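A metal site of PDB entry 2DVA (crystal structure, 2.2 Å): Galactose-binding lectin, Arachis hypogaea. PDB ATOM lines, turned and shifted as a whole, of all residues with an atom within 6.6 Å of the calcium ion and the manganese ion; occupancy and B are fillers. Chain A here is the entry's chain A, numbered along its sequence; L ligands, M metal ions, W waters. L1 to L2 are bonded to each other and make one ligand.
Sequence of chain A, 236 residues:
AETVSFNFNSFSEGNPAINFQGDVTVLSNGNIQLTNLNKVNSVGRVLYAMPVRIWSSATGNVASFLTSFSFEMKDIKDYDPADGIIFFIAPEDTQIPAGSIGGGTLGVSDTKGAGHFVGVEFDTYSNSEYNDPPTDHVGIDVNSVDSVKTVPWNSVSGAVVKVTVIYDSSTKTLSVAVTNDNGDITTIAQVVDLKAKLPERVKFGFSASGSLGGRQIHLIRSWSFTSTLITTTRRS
ND2 of Asn 127 sits at hydrogen-bond distance from O2 of LG2 L2 (2.8 Å).
The backbone NH (N) of Gly 104 sits at hydrogen-bond distance from an oxygen (O2) of LG2 L2.
The side-chain carboxylate (OD1) of Asp 83 is in hydrogen-bond range of an oxygen (O2) of LG2 L2, at 2.6 Å.
The side-chain carboxylate of Glu 121 lies close to the side-chain carboxylate of Asp 141 (2.6 Å).
The backbone carbonyl oxygen of Gly 139 is in hydrogen-bond range of the backbone NH of Glu 121, at 2.8 Å.
Within 4 Å of the calcium ion: Asp 123, Tyr 125, Asn 127 and Asp 132.
The nearest printed residue that does not touch the calcium ion is Gly 104 (4.4 Å).
The calcium ion is bound by the backbone carbonyl oxygen (O) of Tyr 125 (2.5 Å), the side-chain amide oxygen (OD1) of Asn 127 (2.5 Å), the side-chain carboxylate (OD2) of Asp 132 (2.6 Å), water W3 (2.6 Å), the side-chain carboxylate (OD1) of Asp 123 (2.6 Å), water W1 (2.6 Å) and the side-chain carboxylate (OD2) of Asp 123 (2.7 Å).
The calcium ion has seven donor atoms within binding distance.
The manganese ion is bound by OD2 of Asp 123 (2.2 Å), OE2 of Glu 121 (2.2 Å), OD1 of Asp 132 (2.2 Å), water W4 (2.3 Å), water W2 (2.3 Å) and NE2 of His 137 (2.4 Å).
The manganese ion has six donor atoms within binding distance.
Water W2 lies within hydrogen-bond range of the backbone carbonyl oxygen (O) of Val 145 (2.6 Å) and the side-chain carboxylate (OE1) of Glu 121 (2.6 Å).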
ATOM      1  N   ASP A  83     -27.356 -34.098  18.190  1.00  0.00           N
ATOM      2  CA  ASP A  83     -27.667 -33.144  19.265  1.00  0.00           C
ATOM      3  C   ASP A  83     -26.907 -31.820  19.186  1.00  0.00           C
ATOM      4  O   ASP A  83     -27.319 -30.830  19.800  1.00  0.00           O
ATOM      5  CB  ASP A  83     -27.399 -33.801  20.622  1.00  0.00           C
ATOM      6  CG  ASP A  83     -28.561 -34.622  21.107  1.00  0.00           C
ATOM      7  OD1 ASP A  83     -29.446 -34.050  21.773  1.00  0.00           O
ATOM      8  OD2 ASP A  83     -28.600 -35.828  20.803  1.00  0.00           O
ATOM      9  N   GLY A 103     -26.421 -38.088  23.335  1.00  0.00           N
ATOM     10  CA  GLY A 103     -27.551 -37.183  23.331  1.00  0.00           C
ATOM     11  C   GLY A 103     -27.219 -35.771  23.801  1.00  0.00           C
ATOM     12  O   GLY A 103     -26.233 -35.160  23.359  1.00  0.00           O
ATOM     13  N   GLY A 104     -28.037 -35.266  24.720  1.00  0.00           N
ATOM     14  CA  GLY A 104     -27.847 -33.924  25.237  1.00  0.00           C
ATOM     15  C   GLY A 104     -26.576 -33.679  26.032  1.00  0.00           C
ATOM     16  O   GLY A 104     -26.253 -32.526  26.328  1.00  0.00           O
ATOM     17  N   THR A 105     -25.855 -34.747  26.377  1.00  0.00           N
ATOM     18  CA  THR A 105     -24.609 -34.631  27.123  1.00  0.00           C
ATOM     19  C   THR A 105     -23.497 -34.106  26.220  1.00  0.00           C
ATOM     20  O   THR A 105     -22.416 -33.753  26.692  1.00  0.00           O
ATOM     21  CB  THR A 105     -24.152 -35.983  27.693  1.00  0.00           C
ATOM     22  OG1 THR A 105     -23.787 -36.852  26.619  1.00  0.00           O
ATOM     23  CG2 THR A 105     -25.268 -36.639  28.495  1.00  0.00           C
ATOM     24  N   LEU A 106     -23.763 -34.088  24.914  1.00  0.00           N
ATOM     25  CA  LEU A 106     -22.805 -33.630  23.912  1.00  0.00           C
ATOM     26  C   LEU A 106     -21.472 -34.340  23.992  1.00  0.00           C
ATOM     27  O   LEU A 106     -20.462 -33.856  23.450  1.00  0.00           O
ATOM     28  CB  LEU A 106     -22.613 -32.111  24.024  1.00  0.00           C
ATOM     29  CG  LEU A 106     -23.866 -31.268  23.812  1.00  0.00           C
ATOM     30  CD1 LEU A 106     -23.506 -29.787  23.948  1.00  0.00           C
ATOM     31  CD2 LEU A 106     -24.466 -31.554  22.441  1.00  0.00           C
ATOM     32  N   GLU A 121     -21.036 -24.411  23.199  1.00  0.00           N
ATOM     33  CA  GLU A 121     -21.894 -25.366  22.515  1.00  0.00           C
ATOM     34  C   GLU A 121     -22.782 -24.748  21.454  1.00  0.00           C
ATOM     35  O   GLU A 121     -23.141 -23.567  21.524  1.00  0.00           O
ATOM     36  CB  GLU A 121     -22.752 -26.135  23.529  1.00  0.00           C
ATOM     37  CG  GLU A 121     -23.637 -25.221  24.357  1.00  0.00           C
ATOM     38  CD  GLU A 121     -24.747 -25.973  25.057  1.00  0.00           C
ATOM     39  OE1 GLU A 121     -24.450 -26.797  25.945  1.00  0.00           O
ATOM     40  OE2 GLU A 121     -25.914 -25.731  24.709  1.00  0.00           O
ATOM     41  N   ASP A 123     -25.987 -26.061  20.263  1.00  0.00           N
ATOM     42  CA  ASP A 123     -27.063 -26.972  20.577  1.00  0.00           C
ATOM     43  C   ASP A 123     -28.262 -26.962  19.646  1.00  0.00           C
ATOM     44  O   ASP A 123     -28.884 -25.916  19.461  1.00  0.00           O
ATOM     45  CB  ASP A 123     -27.531 -26.640  21.991  1.00  0.00           C
ATOM     46  CG  ASP A 123     -28.035 -27.828  22.704  1.00  0.00           C
ATOM     47  OD1 ASP A 123     -28.586 -28.724  22.031  1.00  0.00           O
ATOM     48  OD2 ASP A 123     -27.908 -27.861  23.943  1.00  0.00           O
ATOM     49  N   THR A 124     -28.621 -28.124  19.096  1.00  0.00           N
ATOM     50  CA  THR A 124     -29.752 -28.207  18.169  1.00  0.00           C
ATOM     51  C   THR A 124     -30.968 -28.992  18.671  1.00  0.00           C
ATOM     52  O   THR A 124     -31.832 -29.375  17.874  1.00  0.00           O
ATOM     53  CB  THR A 124     -29.344 -28.836  16.827  1.00  0.00           C
ATOM     54  OG1 THR A 124     -29.060 -30.227  17.022  1.00  0.00           O
ATOM     55  CG2 THR A 124     -28.103 -28.140  16.276  1.00  0.00           C
ATOM     56  N   TYR A 125     -31.044 -29.250  19.974  1.00  0.00           N
ATOM     57  CA  TYR A 125     -32.176 -29.971  20.539  1.00  0.00           C
ATOM     58  C   TYR A 125     -32.420 -29.480  21.954  1.00  0.00           C
ATOM     59  O   TYR A 125     -31.486 -29.327  22.728  1.00  0.00           O
ATOM     60  CB  TYR A 125     -31.945 -31.481  20.536  1.00  0.00           C
ATOM     61  CG  TYR A 125     -33.081 -32.244  21.176  1.00  0.00           C
ATOM     62  CD1 TYR A 125     -33.099 -32.468  22.555  1.00  0.00           C
ATOM     63  CD2 TYR A 125     -34.175 -32.673  20.424  1.00  0.00           C
ATOM     64  CE1 TYR A 125     -34.180 -33.079  23.171  1.00  0.00           C
ATOM     65  CE2 TYR A 125     -35.278 -33.290  21.033  1.00  0.00           C
ATOM     66  CZ  TYR A 125     -35.277 -33.491  22.410  1.00  0.00           C
ATOM     67  OH  TYR A 125     -36.347 -34.085  23.034  1.00  0.00           O
ATOM     68  N   SER A 126     -33.673 -29.238  22.312  1.00  0.00           N
ATOM     69  CA  SER A 126     -33.974 -28.734  23.653  1.00  0.00           C
ATOM     70  C   SER A 126     -34.159 -29.800  24.742  1.00  0.00           C
ATOM     71  O   SER A 126     -35.251 -30.358  24.887  1.00  0.00           O
ATOM     72  CB  SER A 126     -35.214 -27.852  23.605  1.00  0.00           C
ATOM     73  OG  SER A 126     -35.397 -27.171  24.827  1.00  0.00           O
ATOM     74  N   ASN A 127     -33.097 -30.072  25.494  1.00  0.00           N
ATOM     75  CA  ASN A 127     -33.151 -31.041  26.592  1.00  0.00           C
ATOM     76  C   ASN A 127     -33.575 -30.316  27.861  1.00  0.00           C
ATOM     77  O   ASN A 127     -32.788 -29.610  28.489  1.00  0.00           O
ATOM     78  CB  ASN A 127     -31.792 -31.694  26.844  1.00  0.00           C
ATOM     79  CG  ASN A 127     -31.335 -32.542  25.680  1.00  0.00           C
ATOM     80  OD1 ASN A 127     -30.968 -32.007  24.641  1.00  0.00           O
ATOM     81  ND2 ASN A 127     -31.349 -33.860  25.839  1.00  0.00           N
ATOM     82  N   TYR A 130     -31.677 -30.461  31.064  1.00  0.00           N
ATOM     83  CA  TYR A 130     -30.464 -29.644  31.179  1.00  0.00           C
ATOM     84  C   TYR A 130     -30.832 -28.164  31.107  1.00  0.00           C
ATOM     85  O   TYR A 130     -29.959 -27.310  30.924  1.00  0.00           O
ATOM     86  CB  TYR A 130     -29.466 -29.997  30.080  1.00  0.00           C
ATOM     87  CG  TYR A 130     -29.064 -31.451  30.086  1.00  0.00           C
ATOM     88  CD1 TYR A 130     -28.737 -32.093  31.281  1.00  0.00           C
ATOM     89  CD2 TYR A 130     -29.003 -32.184  28.896  1.00  0.00           C
ATOM     90  CE1 TYR A 130     -28.375 -33.445  31.296  1.00  0.00           C
ATOM     91  CE2 TYR A 130     -28.634 -33.529  28.900  1.00  0.00           C
ATOM     92  CZ  TYR A 130     -28.324 -34.158  30.103  1.00  0.00           C
ATOM     93  OH  TYR A 130     -27.985 -35.491  30.115  1.00  0.00           O
ATOM     94  N   ASN A 131     -32.120 -27.889  31.248  1.00  0.00           N
ATOM     95  CA  ASN A 131     -32.640 -26.529  31.216  1.00  0.00           C
ATOM     96  C   ASN A 131     -32.346 -25.754  29.933  1.00  0.00           C
ATOM     97  O   ASN A 131     -32.152 -24.544  29.969  1.00  0.00           O
ATOM     98  CB  ASN A 131     -32.124 -25.738  32.423  1.00  0.00           C
ATOM     99  CG  ASN A 131     -32.645 -26.280  33.746  1.00  0.00           C
ATOM    100  OD1 ASN A 131     -33.853 -26.340  33.966  1.00  0.00           O
ATOM    101  ND2 ASN A 131     -31.742 -26.683  34.630  1.00  0.00           N
ATOM    102  N   ASP A 132     -32.327 -26.446  28.790  1.00  0.00           N
ATOM    103  CA  ASP A 132     -32.084 -25.782  27.518  1.00  0.00           C
ATOM    104  C   ASP A 132     -33.161 -24.775  27.151  1.00  0.00           C
ATOM    105  O   ASP A 132     -34.319 -24.928  27.532  1.00  0.00           O
ATOM    106  CB  ASP A 132     -32.038 -26.772  26.360  1.00  0.00           C
ATOM    107  CG  ASP A 132     -30.741 -27.500  26.257  1.00  0.00           C
ATOM    108  OD1 ASP A 132     -29.685 -26.897  26.538  1.00  0.00           O
ATOM    109  OD2 ASP A 132     -30.774 -28.683  25.887  1.00  0.00           O
ATOM    110  N   PRO A 133     -32.782 -23.729  26.404  1.00  0.00           N
ATOM    111  CA  PRO A 133     -33.779 -22.726  25.990  1.00  0.00           C
ATOM    112  C   PRO A 133     -34.693 -23.519  25.062  1.00  0.00           C
ATOM    113  O   PRO A 133     -34.391 -24.648  24.707  1.00  0.00           O
ATOM    114  CB  PRO A 133     -32.942 -21.697  25.225  1.00  0.00           C
ATOM    115  CG  PRO A 133     -31.586 -21.834  25.829  1.00  0.00           C
ATOM    116  CD  PRO A 133     -31.432 -23.321  25.998  1.00  0.00           C
ATOM    117  N   HIS A 137     -29.465 -22.967  20.017  1.00  0.00           N
ATOM    118  CA  HIS A 137     -28.738 -21.935  20.724  1.00  0.00           C
ATOM    119  C   HIS A 137     -27.238 -22.187  20.850  1.00  0.00           C
ATOM    120  O   HIS A 137     -26.756 -23.303  20.661  1.00  0.00           O
ATOM    121  CB  HIS A 137     -29.311 -21.797  22.131  1.00  0.00           C
ATOM    122  CG  HIS A 137     -29.334 -23.094  22.889  1.00  0.00           C
ATOM    123  ND1 HIS A 137     -30.261 -24.087  22.654  1.00  0.00           N
ATOM    124  CD2 HIS A 137     -28.501 -23.578  23.847  1.00  0.00           C
ATOM    125  CE1 HIS A 137     -30.001 -25.120  23.429  1.00  0.00           C
ATOM    126  NE2 HIS A 137     -28.946 -24.841  24.158  1.00  0.00           N
ATOM    127  N   GLY A 139     -24.226 -21.773  23.592  1.00  0.00           N
ATOM    128  CA  GLY A 139     -24.106 -21.598  25.020  1.00  0.00           C
ATOM    129  C   GLY A 139     -22.669 -21.683  25.509  1.00  0.00           C
ATOM    130  O   GLY A 139     -21.811 -22.268  24.848  1.00  0.00           O
ATOM    131  N   ASP A 141     -20.534 -23.141  28.429  1.00  0.00           N
ATOM    132  CA  ASP A 141     -20.634 -24.131  29.495  1.00  0.00           C
ATOM    133  C   ASP A 141     -19.417 -24.178  30.415  1.00  0.00           C
ATOM    134  O   ASP A 141     -18.276 -24.047  29.973  1.00  0.00           O
ATOM    135  CB  ASP A 141     -20.844 -25.529  28.893  1.00  0.00           C
ATOM    136  CG  ASP A 141     -22.069 -25.607  27.995  1.00  0.00           C
ATOM    137  OD1 ASP A 141     -22.917 -24.683  28.036  1.00  0.00           O
ATOM    138  OD2 ASP A 141     -22.186 -26.612  27.260  1.00  0.00           O
ATOM    139  N   VAL A 145     -23.579 -29.118  30.995  1.00  0.00           N
ATOM    140  CA  VAL A 145     -24.298 -28.820  29.758  1.00  0.00           C
ATOM    141  C   VAL A 145     -25.503 -27.945  30.065  1.00  0.00           C
ATOM    142  O   VAL A 145     -26.253 -27.567  29.167  1.00  0.00           O
ATOM    143  CB  VAL A 145     -24.748 -30.089  28.994  1.00  0.00           C
ATOM    144  CG1 VAL A 145     -23.537 -30.781  28.382  1.00  0.00           C
ATOM    145  CG2 VAL A 145     -25.499 -31.030  29.912  1.00  0.00           C
ATOM    146  N   ASP A 146     -25.688 -27.630  31.343  1.00  0.00           N
ATOM    147  CA  ASP A 146     -26.748 -26.726  31.766  1.00  0.00           C
ATOM    148  C   ASP A 146     -25.987 -25.411  31.692  1.00  0.00           C
ATOM    149  O   ASP A 146     -25.369 -24.963  32.666  1.00  0.00           O
ATOM    150  CB  ASP A 146     -27.160 -27.009  33.222  1.00  0.00           C
ATOM    151  CG  ASP A 146     -28.324 -26.134  33.675  1.00  0.00           C
ATOM    152  OD1 ASP A 146     -28.439 -24.989  33.181  1.00  0.00           O
ATOM    153  OD2 ASP A 146     -29.125 -26.570  34.535  1.00  0.00           O
ATOM    154  N   SER A 147     -26.010 -24.809  30.509  1.00  0.00           N
ATOM    155  CA  SER A 147     -25.285 -23.579  30.229  1.00  0.00           C
ATOM    156  C   SER A 147     -25.353 -22.433  31.236  1.00  0.00           C
ATOM    157  O   SER A 147     -26.422 -22.095  31.766  1.00  0.00           O
ATOM    158  CB  SER A 147     -25.700 -23.056  28.841  1.00  0.00           C
ATOM    159  OG  SER A 147     -25.343 -23.984  27.827  1.00  0.00           O
ATOM    160  N   THR A 150     -26.840 -18.673  27.502  1.00  0.00           N
ATOM    161  CA  THR A 150     -27.135 -19.067  26.122  1.00  0.00           C
ATOM    162  C   THR A 150     -27.681 -17.890  25.315  1.00  0.00           C
ATOM    163  O   THR A 150     -28.074 -16.869  25.875  1.00  0.00           O
ATOM    164  CB  THR A 150     -28.192 -20.193  26.054  1.00  0.00           C
ATOM    165  OG1 THR A 150     -29.491 -19.658  26.310  1.00  0.00           O
ATOM    166  CG2 THR A 150     -27.883 -21.268  27.068  1.00  0.00           C
HETATM  167  O1  LIG L   1     -37.268 -43.383  20.494  1.00  0.00           O
HETATM  168  C1  LIG L   1     -36.367 -42.294  20.433  1.00  0.00           C
HETATM  169  C2  LIG L   1     -35.978 -41.786  21.818  1.00  0.00           C
HETATM  170  O2  LIG L   1     -35.440 -42.911  22.709  1.00  0.00           O
HETATM  171  C3  LIG L   1     -35.112 -42.569  24.133  1.00  0.00           C
HETATM  172  O3  LIG L   1     -36.320 -42.094  24.783  1.00  0.00           O
HETATM  173  C4  LIG L   1     -37.454 -43.084  25.220  1.00  0.00           C
HETATM  174  C5  LIG L   1     -34.011 -41.495  24.112  1.00  0.00           C
HETATM  175  N1  LIG L   1     -33.785 -41.243  25.493  1.00  0.00           N
HETATM  176  C6  LIG L   1     -32.565 -41.004  26.065  1.00  0.00           C
HETATM  177  O4  LIG L   1     -31.482 -41.412  25.594  1.00  0.00           O
HETATM  178  C7  LIG L   1     -32.550 -40.201  27.353  1.00  0.00           C
HETATM  179  C8  LIG L   1     -34.475 -40.279  23.276  1.00  0.00           C
HETATM  180  O5  LIG L   1     -33.400 -39.409  23.236  1.00  0.00           O
HETATM  181  C9  LIG L   1     -34.865 -40.630  21.780  1.00  0.00           C
HETATM  182  O6  LIG L   1     -33.648 -41.058  21.108  1.00  0.00           O
HETATM  183  C1  LG2 L   2     -33.370 -37.998  23.191  1.00  0.00           C
HETATM  184  C2  LG2 L   2     -32.097 -37.343  23.685  1.00  0.00           C
HETATM  185  C3  LG2 L   2     -31.953 -35.902  23.166  1.00  0.00           C
HETATM  186  C4  LG2 L   2     -32.062 -35.826  21.542  1.00  0.00           C
HETATM  187  C5  LG2 L   2     -33.454 -36.398  21.147  1.00  0.00           C
HETATM  188  C6  LG2 L   2     -34.133 -36.499  19.804  1.00  0.00           C
HETATM  189  O1  LG2 L   2     -32.168 -37.418  25.104  1.00  0.00           O
HETATM  190  O2  LG2 L   2     -30.674 -35.398  23.562  1.00  0.00           O
HETATM  191  O3  LG2 L   2     -31.096 -36.671  20.900  1.00  0.00           O
HETATM  192  O4  LG2 L   2     -33.529 -37.819  21.693  1.00  0.00           O
HETATM  193  O5  LG2 L   2     -35.459 -36.646  19.345  1.00  0.00           O
HETATM  194 CA    CA M   1     -29.479 -30.011  24.094  1.00  0.00          CA
HETATM  195 MN    MN M   2     -27.804 -26.411  25.533  1.00  0.00          MN
HETATM  196  O   HOH W   1     -27.461 -30.403  25.765  1.00  0.00           O
HETATM  197  O   HOH W   2     -26.618 -28.069  26.638  1.00  0.00           O
HETATM  198  O   HOH W   3     -28.529 -31.467  22.187  1.00  0.00           O
HETATM  199  O   HOH W   4     -27.778 -24.713  27.095  1.00  0.00           O
